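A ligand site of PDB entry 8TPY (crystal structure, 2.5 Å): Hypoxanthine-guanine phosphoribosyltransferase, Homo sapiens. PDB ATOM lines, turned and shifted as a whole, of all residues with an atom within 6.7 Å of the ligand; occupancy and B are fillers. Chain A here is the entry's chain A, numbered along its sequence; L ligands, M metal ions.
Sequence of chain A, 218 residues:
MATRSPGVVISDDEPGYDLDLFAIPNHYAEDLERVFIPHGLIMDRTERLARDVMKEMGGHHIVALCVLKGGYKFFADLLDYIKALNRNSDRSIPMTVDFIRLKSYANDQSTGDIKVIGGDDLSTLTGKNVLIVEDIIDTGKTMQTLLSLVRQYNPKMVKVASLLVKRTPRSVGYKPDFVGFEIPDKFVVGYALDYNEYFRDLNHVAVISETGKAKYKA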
ATOM      1  N   GLY A  70       3.575   3.928 -10.005  1.00  0.00           N
ATOM      2  CA  GLY A  70       3.262   3.533 -11.368  1.00  0.00           C
ATOM      3  C   GLY A  70       1.938   2.811 -11.511  1.00  0.00           C
ATOM      4  O   GLY A  70       0.884   3.351 -11.150  1.00  0.00           O
ATOM      5  N   GLU A 134       6.779  -3.355 -13.479  1.00  0.00           N
ATOM      6  CA  GLU A 134       6.586  -1.981 -13.900  1.00  0.00           C
ATOM      7  C   GLU A 134       5.467  -1.926 -14.925  1.00  0.00           C
ATOM      8  O   GLU A 134       5.238  -2.874 -15.684  1.00  0.00           O
ATOM      9  CB  GLU A 134       7.862  -1.383 -14.490  1.00  0.00           C
ATOM     10  CG  GLU A 134       7.722   0.068 -14.911  1.00  0.00           C
ATOM     11  CD  GLU A 134       7.687   1.025 -13.731  1.00  0.00           C
ATOM     12  OE1 GLU A 134       8.543   0.870 -12.831  1.00  0.00           O
ATOM     13  OE2 GLU A 134       6.819   1.912 -13.691  1.00  0.00           O
ATOM     14  N   ASP A 135       4.754  -0.798 -14.950  1.00  0.00           N
ATOM     15  CA  ASP A 135       3.702  -0.617 -15.939  1.00  0.00           C
ATOM     16  C   ASP A 135       4.283  -0.228 -17.291  1.00  0.00           C
ATOM     17  O   ASP A 135       3.959  -0.852 -18.313  1.00  0.00           O
ATOM     18  CB  ASP A 135       2.697   0.438 -15.464  1.00  0.00           C
ATOM     19  CG  ASP A 135       3.369   1.725 -15.021  1.00  0.00           C
ATOM     20  OD1 ASP A 135       4.605   1.730 -14.871  1.00  0.00           O
ATOM     21  OD2 ASP A 135       2.646   2.736 -14.818  1.00  0.00           O
ATOM     22  N   ILE A 136       5.160   0.780 -17.331  1.00  0.00           N
ATOM     23  CA  ILE A 136       5.702   1.278 -18.590  1.00  0.00           C
ATOM     24  C   ILE A 136       7.182   1.605 -18.420  1.00  0.00           C
ATOM     25  O   ILE A 136       7.606   2.141 -17.387  1.00  0.00           O
ATOM     26  CB  ILE A 136       4.939   2.510 -19.096  1.00  0.00           C
ATOM     27  CG1 ILE A 136       5.593   3.017 -20.389  1.00  0.00           C
ATOM     28  CG2 ILE A 136       4.935   3.600 -18.046  1.00  0.00           C
ATOM     29  CD1 ILE A 136       4.601   3.417 -21.467  1.00  0.00           C
ATOM     30  N   ILE A 137       7.952   1.290 -19.453  1.00  0.00           N
ATOM     31  CA  ILE A 137       9.362   1.634 -19.539  1.00  0.00           C
ATOM     32  C   ILE A 137       9.511   2.602 -20.713  1.00  0.00           C
ATOM     33  O   ILE A 137       9.349   2.211 -21.868  1.00  0.00           O
ATOM     34  CB  ILE A 137      10.242   0.391 -19.720  1.00  0.00           C
ATOM     35  CG1 ILE A 137      10.382  -0.331 -18.386  1.00  0.00           C
ATOM     36  CG2 ILE A 137      11.589   0.768 -20.327  1.00  0.00           C
ATOM     37  CD1 ILE A 137      11.307  -1.526 -18.410  1.00  0.00           C
ATOM     38  N   ASP A 138       9.769   3.877 -20.397  1.00  0.00           N
ATOM     39  CA  ASP A 138       9.932   4.920 -21.411  1.00  0.00           C
ATOM     40  C   ASP A 138      11.395   5.012 -21.808  1.00  0.00           C
ATOM     41  O   ASP A 138      11.845   4.309 -22.723  1.00  0.00           O
ATOM     42  CB  ASP A 138       9.402   6.257 -20.880  1.00  0.00           C
ATOM     43  CG  ASP A 138       9.039   7.242 -21.986  1.00  0.00           C
ATOM     44  OD1 ASP A 138       8.902   6.819 -23.163  1.00  0.00           O
ATOM     45  OD2 ASP A 138       8.894   8.451 -21.686  1.00  0.00           O
ATOM     46  N   THR A 139      12.157   5.871 -21.124  1.00  0.00           N
ATOM     47  CA  THR A 139      13.593   5.995 -21.365  1.00  0.00           C
ATOM     48  C   THR A 139      14.406   4.865 -20.743  1.00  0.00           C
ATOM     49  O   THR A 139      15.555   4.645 -21.148  1.00  0.00           O
ATOM     50  CB  THR A 139      14.133   7.323 -20.817  1.00  0.00           C
ATOM     51  OG1 THR A 139      14.127   7.292 -19.382  1.00  0.00           O
ATOM     52  CG2 THR A 139      13.319   8.504 -21.310  1.00  0.00           C
ATOM     53  N   GLY A 140      13.851   4.165 -19.751  1.00  0.00           N
ATOM     54  CA  GLY A 140      14.583   3.112 -19.077  1.00  0.00           C
ATOM     55  C   GLY A 140      15.497   3.567 -17.973  1.00  0.00           C
ATOM     56  O   GLY A 140      16.182   2.728 -17.368  1.00  0.00           O
ATOM     57  N   LYS A 141      15.557   4.868 -17.679  1.00  0.00           N
ATOM     58  CA  LYS A 141      16.444   5.352 -16.629  1.00  0.00           C
ATOM     59  C   LYS A 141      15.982   4.902 -15.248  1.00  0.00           C
ATOM     60  O   LYS A 141      16.810   4.752 -14.339  1.00  0.00           O
ATOM     61  CB  LYS A 141      16.569   6.870 -16.692  1.00  0.00           C
ATOM     62  N   THR A 142      14.685   4.682 -15.075  1.00  0.00           N
ATOM     63  CA  THR A 142      14.186   4.178 -13.797  1.00  0.00           C
ATOM     64  C   THR A 142      14.689   2.760 -13.536  1.00  0.00           C
ATOM     65  O   THR A 142      15.252   2.475 -12.475  1.00  0.00           O
ATOM     66  CB  THR A 142      12.653   4.216 -13.769  1.00  0.00           C
ATOM     67  OG1 THR A 142      12.209   5.568 -13.921  1.00  0.00           O
ATOM     68  CG2 THR A 142      12.131   3.659 -12.455  1.00  0.00           C
ATOM     69  N   MET A 143      14.489   1.843 -14.484  1.00  0.00           N
ATOM     70  CA  MET A 143      14.909   0.461 -14.269  1.00  0.00           C
ATOM     71  C   MET A 143      16.423   0.350 -14.168  1.00  0.00           C
ATOM     72  O   MET A 143      16.939  -0.337 -13.289  1.00  0.00           O
ATOM     73  CB  MET A 143      14.391  -0.447 -15.387  1.00  0.00           C
ATOM     74  CG  MET A 143      13.004  -0.996 -15.102  1.00  0.00           C
ATOM     75  SD  MET A 143      12.909  -1.664 -13.428  1.00  0.00           S
ATOM     76  CE  MET A 143      11.285  -1.075 -12.943  1.00  0.00           C
ATOM     77  N   LEU A 164       4.327  -2.441 -20.675  1.00  0.00           N
ATOM     78  CA  LEU A 164       4.571  -1.703 -21.904  1.00  0.00           C
ATOM     79  C   LEU A 164       6.034  -1.281 -21.968  1.00  0.00           C
ATOM     80  O   LEU A 164       6.575  -0.745 -20.991  1.00  0.00           O
ATOM     81  CB  LEU A 164       3.696  -0.448 -21.996  1.00  0.00           C
ATOM     82  CG  LEU A 164       2.210  -0.559 -21.706  1.00  0.00           C
ATOM     83  CD1 LEU A 164       1.640   0.839 -21.713  1.00  0.00           C
ATOM     84  CD2 LEU A 164       1.511  -1.451 -22.715  1.00  0.00           C
ATOM     85  N   LYS A 166       8.097   1.264 -24.473  1.00  0.00           N
ATOM     86  CA  LYS A 166       7.993   2.231 -25.562  1.00  0.00           C
ATOM     87  C   LYS A 166       9.225   2.178 -26.450  1.00  0.00           C
ATOM     88  O   LYS A 166      10.357   2.211 -25.958  1.00  0.00           O
ATOM     89  CB  LYS A 166       7.821   3.650 -25.004  1.00  0.00           C
ATOM     90  CG  LYS A 166       6.424   3.960 -24.509  1.00  0.00           C
ATOM     91  CD  LYS A 166       6.355   5.368 -23.953  1.00  0.00           C
ATOM     92  CE  LYS A 166       5.320   6.192 -24.676  1.00  0.00           C
ATOM     93  NZ  LYS A 166       5.345   7.619 -24.239  1.00  0.00           N
ATOM     94  N   ARG A 170      14.650   8.104 -27.182  1.00  0.00           N
ATOM     95  CA  ARG A 170      15.022   8.531 -25.841  1.00  0.00           C
ATOM     96  C   ARG A 170      15.399   7.353 -24.948  1.00  0.00           C
ATOM     97  O   ARG A 170      15.692   7.568 -23.768  1.00  0.00           O
ATOM     98  CB  ARG A 170      13.875   9.318 -25.196  1.00  0.00           C
ATOM     99  CG  ARG A 170      13.479  10.559 -25.978  1.00  0.00           C
ATOM    100  CD  ARG A 170      12.245  11.230 -25.411  1.00  0.00           C
ATOM    101  NE  ARG A 170      11.037  10.445 -25.623  1.00  0.00           N
ATOM    102  CZ  ARG A 170      10.368   9.808 -24.674  1.00  0.00           C
ATOM    103  NH1 ARG A 170      10.741   9.871 -23.411  1.00  0.00           N
ATOM    104  NH2 ARG A 170       9.295   9.097 -25.005  1.00  0.00           N
ATOM    105  N   ILE A 183       5.303  -0.828 -27.845  1.00  0.00           N
ATOM    106  CA  ILE A 183       4.329   0.106 -28.425  1.00  0.00           C
ATOM    107  C   ILE A 183       5.097   1.261 -29.057  1.00  0.00           C
ATOM    108  O   ILE A 183       6.275   1.526 -28.709  1.00  0.00           O
ATOM    109  CB  ILE A 183       3.308   0.621 -27.379  1.00  0.00           C
ATOM    110  CG1 ILE A 183       4.004   1.449 -26.316  1.00  0.00           C
ATOM    111  CG2 ILE A 183       2.590  -0.571 -26.754  1.00  0.00           C
ATOM    112  CD1 ILE A 183       3.054   2.214 -25.418  1.00  0.00           C
ATOM    113  N   ASP A 185       6.054   5.280 -29.852  1.00  0.00           N
ATOM    114  CA  ASP A 185       6.385   6.357 -28.926  1.00  0.00           C
ATOM    115  C   ASP A 185       5.314   7.441 -28.980  1.00  0.00           C
ATOM    116  O   ASP A 185       5.515   8.546 -29.492  1.00  0.00           O
ATOM    117  CB  ASP A 185       7.767   6.928 -29.238  1.00  0.00           C
ATOM    118  CG  ASP A 185       8.226   7.915 -28.188  1.00  0.00           C
ATOM    119  OD1 ASP A 185       7.570   8.003 -27.130  1.00  0.00           O
ATOM    120  OD2 ASP A 185       9.237   8.607 -28.439  1.00  0.00           O
ATOM    121  N   LYS A 186       4.156   7.105 -28.425  1.00  0.00           N
ATOM    122  CA  LYS A 186       3.060   8.048 -28.304  1.00  0.00           C
ATOM    123  C   LYS A 186       2.593   8.035 -26.853  1.00  0.00           C
ATOM    124  O   LYS A 186       2.946   7.150 -26.074  1.00  0.00           O
ATOM    125  CB  LYS A 186       1.928   7.695 -29.278  1.00  0.00           C
ATOM    126  CG  LYS A 186       2.433   7.299 -30.685  1.00  0.00           C
ATOM    127  CD  LYS A 186       2.635   8.498 -31.627  1.00  0.00           C
ATOM    128  CE  LYS A 186       3.976   8.454 -32.415  1.00  0.00           C
ATOM    129  NZ  LYS A 186       4.292   7.166 -33.124  1.00  0.00           N
ATOM    130  N   PHE A 187       1.827   9.055 -26.459  1.00  0.00           N
ATOM    131  CA  PHE A 187       1.402   9.196 -25.071  1.00  0.00           C
ATOM    132  C   PHE A 187       0.112   8.407 -24.851  1.00  0.00           C
ATOM    133  O   PHE A 187      -0.928   8.729 -25.442  1.00  0.00           O
ATOM    134  CB  PHE A 187       1.222  10.657 -24.678  1.00  0.00           C
ATOM    135  CG  PHE A 187       1.274  10.883 -23.198  1.00  0.00           C
ATOM    136  CD1 PHE A 187       2.493  11.021 -22.548  1.00  0.00           C
ATOM    137  CD2 PHE A 187       0.115  10.938 -22.439  1.00  0.00           C
ATOM    138  CE1 PHE A 187       2.554  11.215 -21.184  1.00  0.00           C
ATOM    139  CE2 PHE A 187       0.163  11.135 -21.070  1.00  0.00           C
ATOM    140  CZ  PHE A 187       1.392  11.268 -20.434  1.00  0.00           C
ATOM    141  N   VAL A 188       0.175   7.393 -24.000  1.00  0.00           N
ATOM    142  CA  VAL A 188      -0.916   6.451 -23.798  1.00  0.00           C
ATOM    143  C   VAL A 188      -1.465   6.601 -22.377  1.00  0.00           C
ATOM    144  O   VAL A 188      -0.726   6.896 -21.436  1.00  0.00           O
ATOM    145  CB  VAL A 188      -0.457   5.003 -24.057  1.00  0.00           C
ATOM    146  CG1 VAL A 188      -0.165   4.797 -25.541  1.00  0.00           C
ATOM    147  CG2 VAL A 188       0.779   4.670 -23.226  1.00  0.00           C
ATOM    148  N   VAL A 189      -2.776   6.407 -22.240  1.00  0.00           N
ATOM    149  CA  VAL A 189      -3.443   6.402 -20.949  1.00  0.00           C
ATOM    150  C   VAL A 189      -4.371   5.194 -20.896  1.00  0.00           C
ATOM    151  O   VAL A 189      -4.634   4.541 -21.899  1.00  0.00           O
ATOM    152  CB  VAL A 189      -4.226   7.708 -20.669  1.00  0.00           C
ATOM    153  CG1 VAL A 189      -3.280   8.882 -20.619  1.00  0.00           C
ATOM    154  CG2 VAL A 189      -5.301   7.921 -21.725  1.00  0.00           C
ATOM    155  N   GLY A 190      -4.873   4.912 -19.695  1.00  0.00           N
ATOM    156  CA  GLY A 190      -5.775   3.800 -19.459  1.00  0.00           C
ATOM    157  C   GLY A 190      -5.049   2.593 -18.869  1.00  0.00           C
ATOM    158  O   GLY A 190      -3.852   2.401 -19.023  1.00  0.00           O
ATOM    159  N   ALA A 192      -4.031   1.263 -15.460  1.00  0.00           N
ATOM    160  CA  ALA A 192      -2.788   1.471 -14.730  1.00  0.00           C
ATOM    161  C   ALA A 192      -1.976   2.699 -15.179  1.00  0.00           C
ATOM    162  O   ALA A 192      -1.044   3.085 -14.472  1.00  0.00           O
ATOM    163  CB  ALA A 192      -1.895   0.226 -14.848  1.00  0.00           C
ATOM    164  N   LEU A 193      -2.289   3.307 -16.323  1.00  0.00           N
ATOM    165  CA  LEU A 193      -1.597   4.507 -16.796  1.00  0.00           C
ATOM    166  C   LEU A 193      -2.513   5.710 -16.655  1.00  0.00           C
ATOM    167  O   LEU A 193      -3.386   5.941 -17.493  1.00  0.00           O
ATOM    168  CB  LEU A 193      -1.142   4.374 -18.241  1.00  0.00           C
ATOM    169  CG  LEU A 193      -0.054   3.361 -18.505  1.00  0.00           C
ATOM    170  CD1 LEU A 193       0.400   3.503 -19.934  1.00  0.00           C
ATOM    171  CD2 LEU A 193       1.093   3.576 -17.540  1.00  0.00           C
ATOM    172  N   ASP A 194      -2.294   6.518 -15.627  1.00  0.00           N
ATOM    173  CA  ASP A 194      -3.083   7.729 -15.448  1.00  0.00           C
ATOM    174  C   ASP A 194      -2.353   8.942 -16.028  1.00  0.00           C
ATOM    175  O   ASP A 194      -1.181   8.891 -16.394  1.00  0.00           O
ATOM    176  CB  ASP A 194      -3.392   7.959 -13.965  1.00  0.00           C
ATOM    177  CG  ASP A 194      -2.181   8.419 -13.187  1.00  0.00           C
ATOM    178  OD1 ASP A 194      -1.272   7.592 -12.972  1.00  0.00           O
ATOM    179  OD2 ASP A 194      -2.135   9.610 -12.821  1.00  0.00           O
ATOM    180  N   TYR A 195      -3.105  10.040 -16.108  1.00  0.00           N
ATOM    181  CA  TYR A 195      -2.578  11.342 -16.526  1.00  0.00           C
ATOM    182  C   TYR A 195      -3.107  12.350 -15.506  1.00  0.00           C
ATOM    183  O   TYR A 195      -4.271  12.738 -15.558  1.00  0.00           O
ATOM    184  CB  TYR A 195      -2.997  11.678 -17.948  1.00  0.00           C
ATOM    185  CG  TYR A 195      -2.571  13.054 -18.417  1.00  0.00           C
ATOM    186  CD1 TYR A 195      -1.226  13.374 -18.549  1.00  0.00           C
ATOM    187  CD2 TYR A 195      -3.512  14.030 -18.732  1.00  0.00           C
ATOM    188  CE1 TYR A 195      -0.833  14.637 -18.983  1.00  0.00           C
ATOM    189  CE2 TYR A 195      -3.130  15.285 -19.170  1.00  0.00           C
ATOM    190  CZ  TYR A 195      -1.788  15.578 -19.293  1.00  0.00           C
ATOM    191  OH  TYR A 195      -1.402  16.836 -19.722  1.00  0.00           O
HETATM  192  C1  LIG L   1       5.421   9.453 -17.515  1.00  0.00           C
HETATM  193  C2  LIG L   1       4.207   8.066 -20.480  1.00  0.00           C
HETATM  194  C3  LIG L   1       6.648  10.387 -17.477  1.00  0.00           C
HETATM  195  C4  LIG L   1       8.146  10.492 -15.656  1.00  0.00           C
HETATM  196  C5  LIG L   1       9.712   5.722 -16.708  1.00  0.00           C
HETATM  197  C6  LIG L   1       9.340   6.994 -15.928  1.00  0.00           C
HETATM  198  C7  LIG L   1       7.772   7.065 -16.053  1.00  0.00           C
HETATM  199  C8  LIG L   1       5.729   8.325 -16.490  1.00  0.00           C
HETATM  200  C9  LIG L   1       6.125   8.693 -19.746  1.00  0.00           C
HETATM  201  C10 LIG L   1       4.031   8.531 -19.197  1.00  0.00           C
HETATM  202  C11 LIG L   1       2.997   7.544 -21.262  1.00  0.00           C
HETATM  203  C12 LIG L   1       1.538   8.032 -19.307  1.00  0.00           C
HETATM  204  C13 LIG L   1       7.641   9.718 -16.863  1.00  0.00           C
HETATM  205  N1  LIG L   1       7.036   8.282 -16.441  1.00  0.00           N
HETATM  206  N2  LIG L   1       5.215   8.914 -18.764  1.00  0.00           N
HETATM  207  N3  LIG L   1       5.500   8.181 -20.786  1.00  0.00           N
HETATM  208  N4  LIG L   1       1.702   7.545 -20.657  1.00  0.00           N
HETATM  209  N5  LIG L   1       0.198   8.025 -18.693  1.00  0.00           N
HETATM  210  N6  LIG L   1       2.689   8.534 -18.552  1.00  0.00           N
HETATM  211  O1  LIG L   1      11.438   7.089 -18.494  1.00  0.00           O
HETATM  212  O2  LIG L   1      12.345   6.231 -16.288  1.00  0.00           O
HETATM  213  O3  LIG L   1      11.823   4.657 -18.158  1.00  0.00           O
HETATM  214  O4  LIG L   1       3.145   7.136 -22.385  1.00  0.00           O
HETATM  215  O5  LIG L   1       7.853   9.893 -14.428  1.00  0.00           O
HETATM  216  O6  LIG L   1       7.088   6.094 -15.786  1.00  0.00           O
HETATM  217  P1  LIG L   1      11.422   5.931 -17.469  1.00  0.00           P
HETATM  218 MG    MG M   1       5.389   3.211 -13.161  1.00  0.00          MG
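OG1 of Thr 142 is in hydrogen-bond range of O2 of the ligand (2.5 Å). An oxygen (O3) of the ligand lies within hydrogen-bond range of the backbone NH (N) of Gly 140 (2.6 Å). The side-chain hydroxyl of Thr 139 sits at hydrogen-bond distance from an oxygen (O1) of the ligand. N of Asp 138 is in hydrogen-bond range of O3 of the ligand. The side-chain amino group of Lys 166 is in hydrogen-bond range of an oxygen (O4) of the ligand (2.9 Å). An oxygen (O4) of the ligand is in hydrogen-bond range of the backbone NH (N) of Val 188, at 3.4 Å. The backbone NH (N) of Thr 139 sits at hydrogen-bond distance from an oxygen (O1) of the ligand (3.0 Å). The backbone carbonyl oxygen of Asp 194 lies within hydrogen-bond range of a nitrogen (N5) of the ligand, 2.8 Å away. An oxygen (O2) of the ligand lies within hydrogen-bond range of the backbone NH (N) of Thr 142 (3.1 Å). A nitrogen (N4) of the ligand lies within hydrogen-bond range of the backbone carbonyl oxygen (O) of Val 188 (2.6 Å).
Ile 136 touches the ligand. Lys 141 touches the ligand. Lys 186 touches the ligand. Phe 187 touches the ligand. CB of Leu 193 touches N5 of the ligand (3.9 Å).
The side-chain carboxylate (OD1) of Asp 185 lies within salt-bridge range of the side-chain amino group (NZ) of Lys 166, at 3.7 Å. The side-chain hydroxyl (OG1) of Thr 139 sits close to the backbone NH (N) of Lys 141 (3.3 Å). The side-chain amino group (NZ) of Lys 166 lies close to the backbone carbonyl oxygen (O) of Lys 186 (3.1 Å). OD2 of Asp 138 is in salt-bridge range of NH1 of Arg 170, 2.9 Å away. N of Lys 166 is in hydrogen-bond range of O of Ile 137, at 3.0 Å. The side-chain carboxylate (OD1) of Asp 138 is in salt-bridge range of the side-chain amino group (NZ) of Lys 166 (3.8 Å).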
